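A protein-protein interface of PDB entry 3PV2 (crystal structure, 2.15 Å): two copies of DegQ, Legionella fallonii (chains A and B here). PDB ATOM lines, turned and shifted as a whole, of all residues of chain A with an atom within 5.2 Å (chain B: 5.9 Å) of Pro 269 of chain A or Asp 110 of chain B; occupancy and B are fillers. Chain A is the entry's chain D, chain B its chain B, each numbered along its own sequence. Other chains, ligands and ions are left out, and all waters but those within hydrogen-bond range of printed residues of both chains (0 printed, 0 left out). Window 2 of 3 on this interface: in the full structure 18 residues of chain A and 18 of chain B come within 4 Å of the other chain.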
ATOM      1  N   LEU A 267      12.221 -20.901  22.264  1.00  0.00           N
ATOM      2  CA  LEU A 267      13.006 -22.080  22.434  1.00  0.00           C
ATOM      3  C   LEU A 267      12.104 -23.260  22.096  1.00  0.00           C
ATOM      4  O   LEU A 267      11.319 -23.708  22.923  1.00  0.00           O
ATOM      5  CB  LEU A 267      13.566 -22.202  23.838  1.00  0.00           C
ATOM      6  CG  LEU A 267      14.531 -23.365  23.898  1.00  0.00           C
ATOM      7  CD1 LEU A 267      15.811 -23.151  22.996  1.00  0.00           C
ATOM      8  CD2 LEU A 267      14.906 -23.646  25.363  1.00  0.00           C
ATOM      9  N   THR A 268      12.213 -23.720  20.845  1.00  0.00           N
ATOM     10  CA  THR A 268      11.581 -24.946  20.419  1.00  0.00           C
ATOM     11  C   THR A 268      12.491 -26.103  20.820  1.00  0.00           C
ATOM     12  O   THR A 268      13.699 -25.927  20.998  1.00  0.00           O
ATOM     13  CB  THR A 268      11.505 -25.023  18.884  1.00  0.00           C
ATOM     14  OG1 THR A 268      12.822 -25.109  18.398  1.00  0.00           O
ATOM     15  CG2 THR A 268      10.891 -23.825  18.260  1.00  0.00           C
ATOM     16  N   PRO A 269      11.952 -27.312  20.859  1.00  0.00           N
ATOM     17  CA  PRO A 269      12.669 -28.565  21.097  1.00  0.00           C
ATOM     18  C   PRO A 269      13.954 -28.798  20.299  1.00  0.00           C
ATOM     19  O   PRO A 269      15.024 -29.109  20.886  1.00  0.00           O
ATOM     20  CB  PRO A 269      11.619 -29.597  20.691  1.00  0.00           C
ATOM     21  CG  PRO A 269      10.342 -28.992  21.318  1.00  0.00           C
ATOM     22  CD  PRO A 269      10.493 -27.525  20.869  1.00  0.00           C
ATOM     23  N   GLU A 270      13.851 -28.637  18.988  1.00  0.00           N
ATOM     24  CA  GLU A 270      15.000 -28.884  18.144  1.00  0.00           C
ATOM     25  C   GLU A 270      16.119 -27.888  18.465  1.00  0.00           C
ATOM     26  O   GLU A 270      17.331 -28.200  18.310  1.00  0.00           O
ATOM     27  CB  GLU A 270      14.629 -28.927  16.640  1.00  0.00           C
ATOM     28  CG  GLU A 270      13.803 -27.763  16.061  1.00  0.00           C
ATOM     29  CD  GLU A 270      13.610 -27.861  14.536  1.00  0.00           C
ATOM     30  OE1 GLU A 270      13.382 -26.811  13.889  1.00  0.00           O
ATOM     31  OE2 GLU A 270      13.713 -28.981  13.975  1.00  0.00           O
ATOM     32  N   LEU A 271      15.727 -26.703  18.939  1.00  0.00           N
ATOM     33  CA  LEU A 271      16.721 -25.647  19.184  1.00  0.00           C
ATOM     34  C   LEU A 271      17.321 -26.052  20.553  1.00  0.00           C
ATOM     35  O   LEU A 271      18.524 -26.041  20.752  1.00  0.00           O
ATOM     36  CB  LEU A 271      16.091 -24.219  19.136  1.00  0.00           C
ATOM     37  CG  LEU A 271      16.536 -23.090  18.207  1.00  0.00           C
ATOM     38  CD1 LEU A 271      17.547 -23.549  17.227  1.00  0.00           C
ATOM     39  CD2 LEU A 271      15.393 -22.403  17.475  1.00  0.00           C
ATOM     40  N   ALA A 272      16.482 -26.459  21.476  1.00  0.00           N
ATOM     41  CA  ALA A 272      16.977 -27.005  22.773  1.00  0.00           C
ATOM     42  C   ALA A 272      18.097 -28.058  22.566  1.00  0.00           C
ATOM     43  O   ALA A 272      19.236 -27.901  23.081  1.00  0.00           O
ATOM     44  CB  ALA A 272      15.858 -27.522  23.544  1.00  0.00           C
ATOM     45  N   GLN A 273      17.815 -29.048  21.715  1.00  0.00           N
ATOM     46  CA  GLN A 273      18.712 -30.178  21.482  1.00  0.00           C
ATOM     47  C   GLN A 273      19.945 -29.711  20.788  1.00  0.00           C
ATOM     48  O   GLN A 273      21.073 -30.105  21.133  1.00  0.00           O
ATOM     49  CB  GLN A 273      17.997 -31.279  20.671  1.00  0.00           C
ATOM     50  CG  GLN A 273      16.889 -32.038  21.553  1.00  0.00           C
ATOM     51  CD  GLN A 273      15.815 -32.890  20.773  1.00  0.00           C
ATOM     52  OE1 GLN A 273      15.478 -32.620  19.586  1.00  0.00           O
ATOM     53  NE2 GLN A 273      15.257 -33.899  21.475  1.00  0.00           N
ATOM     54  N   ALA A 274      19.730 -28.848  19.802  1.00  0.00           N
ATOM     55  CA  ALA A 274      20.800 -28.259  19.089  1.00  0.00           C
ATOM     56  C   ALA A 274      21.806 -27.517  19.981  1.00  0.00           C
ATOM     57  O   ALA A 274      22.985 -27.385  19.605  1.00  0.00           O
ATOM     58  CB  ALA A 274      20.240 -27.329  18.035  1.00  0.00           C
ATOM     59  N   GLU A 279      14.951 -31.785  25.531  1.00  0.00           N
ATOM     60  CA  GLU A 279      14.028 -31.398  24.484  1.00  0.00           C
ATOM     61  C   GLU A 279      12.838 -30.648  25.018  1.00  0.00           C
ATOM     62  O   GLU A 279      12.206 -29.893  24.311  1.00  0.00           O
ATOM     63  CB  GLU A 279      13.555 -32.619  23.703  1.00  0.00           C
ATOM     64  CG  GLU A 279      12.072 -32.583  23.294  1.00  0.00           C
ATOM     65  CD  GLU A 279      11.621 -33.823  22.531  1.00  0.00           C
ATOM     66  OE1 GLU A 279      11.808 -33.860  21.289  1.00  0.00           O
ATOM     67  OE2 GLU A 279      11.060 -34.743  23.188  1.00  0.00           O
ATOM     68  N   LEU B 108       4.773 -28.561  12.329  1.00  0.00           N
ATOM     69  CA  LEU B 108       4.200 -29.287  13.430  1.00  0.00           C
ATOM     70  C   LEU B 108       4.167 -28.407  14.643  1.00  0.00           C
ATOM     71  O   LEU B 108       4.878 -27.431  14.747  1.00  0.00           O
ATOM     72  CB  LEU B 108       5.074 -30.499  13.803  1.00  0.00           C
ATOM     73  CG  LEU B 108       5.455 -31.497  12.732  1.00  0.00           C
ATOM     74  CD1 LEU B 108       6.224 -32.709  13.327  1.00  0.00           C
ATOM     75  CD2 LEU B 108       4.235 -31.981  11.944  1.00  0.00           C
ATOM     76  N   GLN B 109       3.415 -28.841  15.621  1.00  0.00           N
ATOM     77  CA  GLN B 109       3.308 -28.113  16.836  1.00  0.00           C
ATOM     78  C   GLN B 109       4.662 -28.016  17.520  1.00  0.00           C
ATOM     79  O   GLN B 109       5.001 -26.980  18.029  1.00  0.00           O
ATOM     80  CB  GLN B 109       2.326 -28.835  17.715  1.00  0.00           C
ATOM     81  CG  GLN B 109       2.155 -28.250  19.049  1.00  0.00           C
ATOM     82  CD  GLN B 109       1.805 -29.313  20.038  1.00  0.00           C
ATOM     83  OE1 GLN B 109       0.678 -29.355  20.553  1.00  0.00           O
ATOM     84  NE2 GLN B 109       2.764 -30.211  20.292  1.00  0.00           N
ATOM     85  N   ASP B 110       5.453 -29.078  17.467  1.00  0.00           N
ATOM     86  CA  ASP B 110       6.767 -29.082  18.102  1.00  0.00           C
ATOM     87  C   ASP B 110       7.798 -28.177  17.408  1.00  0.00           C
ATOM     88  O   ASP B 110       8.919 -28.051  17.864  1.00  0.00           O
ATOM     89  CB  ASP B 110       7.303 -30.508  18.284  1.00  0.00           C
ATOM     90  CG  ASP B 110       7.744 -31.142  16.995  1.00  0.00           C
ATOM     91  OD1 ASP B 110       8.118 -30.402  16.072  1.00  0.00           O
ATOM     92  OD2 ASP B 110       7.724 -32.386  16.915  1.00  0.00           O
ATOM     93  N   GLY B 111       7.425 -27.577  16.289  1.00  0.00           N
ATOM     94  CA  GLY B 111       8.290 -26.613  15.612  1.00  0.00           C
ATOM     95  C   GLY B 111       9.026 -27.039  14.344  1.00  0.00           C
ATOM     96  O   GLY B 111       9.546 -26.200  13.621  1.00  0.00           O
ATOM     97  N   ARG B 112       9.077 -28.322  14.042  1.00  0.00           N
ATOM     98  CA  ARG B 112       9.798 -28.757  12.844  1.00  0.00           C
ATOM     99  C   ARG B 112       9.042 -28.289  11.596  1.00  0.00           C
ATOM    100  O   ARG B 112       7.815 -28.354  11.599  1.00  0.00           O
ATOM    101  CB  ARG B 112       9.899 -30.273  12.823  1.00  0.00           C
ATOM    102  CG  ARG B 112      10.619 -30.889  14.004  1.00  0.00           C
ATOM    103  CD  ARG B 112      10.663 -32.419  13.899  1.00  0.00           C
ATOM    104  NE  ARG B 112       9.566 -33.051  14.635  1.00  0.00           N
ATOM    105  CZ  ARG B 112       9.148 -34.309  14.474  1.00  0.00           C
ATOM    106  NH1 ARG B 112       9.737 -35.116  13.597  1.00  0.00           N
ATOM    107  NH2 ARG B 112       8.128 -34.771  15.202  1.00  0.00           N
ATOM    108  N   ASN B 136       8.313 -39.504  15.501  1.00  0.00           N
ATOM    109  CA  ASN B 136       7.812 -38.783  16.662  1.00  0.00           C
ATOM    110  C   ASN B 136       6.569 -38.012  16.231  1.00  0.00           C
ATOM    111  O   ASN B 136       6.425 -36.847  16.573  1.00  0.00           O
ATOM    112  CB  ASN B 136       8.880 -37.797  17.155  1.00  0.00           C
ATOM    113  CG  ASN B 136       8.792 -37.484  18.644  1.00  0.00           C
ATOM    114  OD1 ASN B 136       9.813 -37.480  19.316  1.00  0.00           O
ATOM    115  ND2 ASN B 136       7.591 -37.197  19.161  1.00  0.00           N
ATOM    116  N   LEU B 163       5.188 -21.429  13.112  1.00  0.00           N
ATOM    117  CA  LEU B 163       6.374 -21.318  13.992  1.00  0.00           C
ATOM    118  C   LEU B 163       6.545 -20.070  14.893  1.00  0.00           C
ATOM    119  O   LEU B 163       6.906 -20.238  16.060  1.00  0.00           O
ATOM    120  CB  LEU B 163       7.678 -21.569  13.218  1.00  0.00           C
ATOM    121  CG  LEU B 163       8.889 -22.080  14.043  1.00  0.00           C
ATOM    122  CD1 LEU B 163       9.437 -21.027  15.033  1.00  0.00           C
ATOM    123  CD2 LEU B 163       8.569 -23.377  14.780  1.00  0.00           C
ATOM    124  N   PHE B 166       4.919 -20.263  18.259  1.00  0.00           N
ATOM    125  CA  PHE B 166       5.215 -21.594  18.810  1.00  0.00           C
ATOM    126  C   PHE B 166       4.715 -21.795  20.251  1.00  0.00           C
ATOM    127  O   PHE B 166       4.977 -20.970  21.117  1.00  0.00           O
ATOM    128  CB  PHE B 166       6.723 -21.864  18.761  1.00  0.00           C
ATOM    129  CG  PHE B 166       7.159 -23.024  19.613  1.00  0.00           C
ATOM    130  CD1 PHE B 166       7.489 -22.820  20.962  1.00  0.00           C
ATOM    131  CD2 PHE B 166       7.218 -24.321  19.068  1.00  0.00           C
ATOM    132  CE1 PHE B 166       7.894 -23.889  21.766  1.00  0.00           C
ATOM    133  CE2 PHE B 166       7.620 -25.399  19.851  1.00  0.00           C
ATOM    134  CZ  PHE B 166       7.969 -25.190  21.201  1.00  0.00           C
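The side-chain carboxylate of Asp 110 of chain B lies within salt-bridge range of the guanidinium group of Arg 112 of chain B. NH2 of Arg 112 of chain B is in hydrogen-bond range of O of Asn 136 of chain B. The side-chain hydroxyl (OG1) of Thr 268 of chain A lies within hydrogen-bond range of the backbone NH (N) of Leu 271 of chain A, at 3.4 Å.
Among the printed residues, merely in contact across the chains: Pro 269 of chain A with Asp 110 of chain B (3.4 Å), Pro 269 of chain A with Phe 166 of chain B (3.5 Å), Leu 267 of chain A with Phe 166 of chain B (3.6 Å), Glu 270 of chain A with Arg 112 of chain B (3.6 Å), Thr 268 of chain A with Phe 166 of chain B (3.7 Å) and Glu 270 of chain A with Gly 111 of chain B (3.9 Å).
Pro 269 of chain A touches just these residues of chain B: Asp 110 and Phe 166. Printed residues of chain B within 4 Å of Glu 270 of chain A: Gly 111 and Arg 112. Of chain A, only Pro 269 (3.4 Å) comes within 4 Å of Asp 110 of chain B. Of the printed residues of chain A, Gly 111 of chain B touches Glu 270. The nearest residue of chain A that does not touch Asp 110 of chain B is Thr 268 of chain A (4.1 Å). The nearest printed residue of chain B that does not touch Leu 267 of chain A is Asp 110 of chain B (7.1 Å).
Printed residues of chain B that touch a printed residue of chain A: Asp 110, Gly 111, Arg 112 and Phe 166. Printed residues of chain A that touch a printed residue of chain B: Leu 267, Thr 268, Pro 269 and Glu 270. Hydrophobic or aromatic side chains of chain A that line the printed part of chain B: Pro 269. Among the printed residues, 6 pairs touch across the chains.
No position is printed for both chains. Of the 6 pairs that touch across the chains among the printed residues, none has its exchanged pair printed and touching as well.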
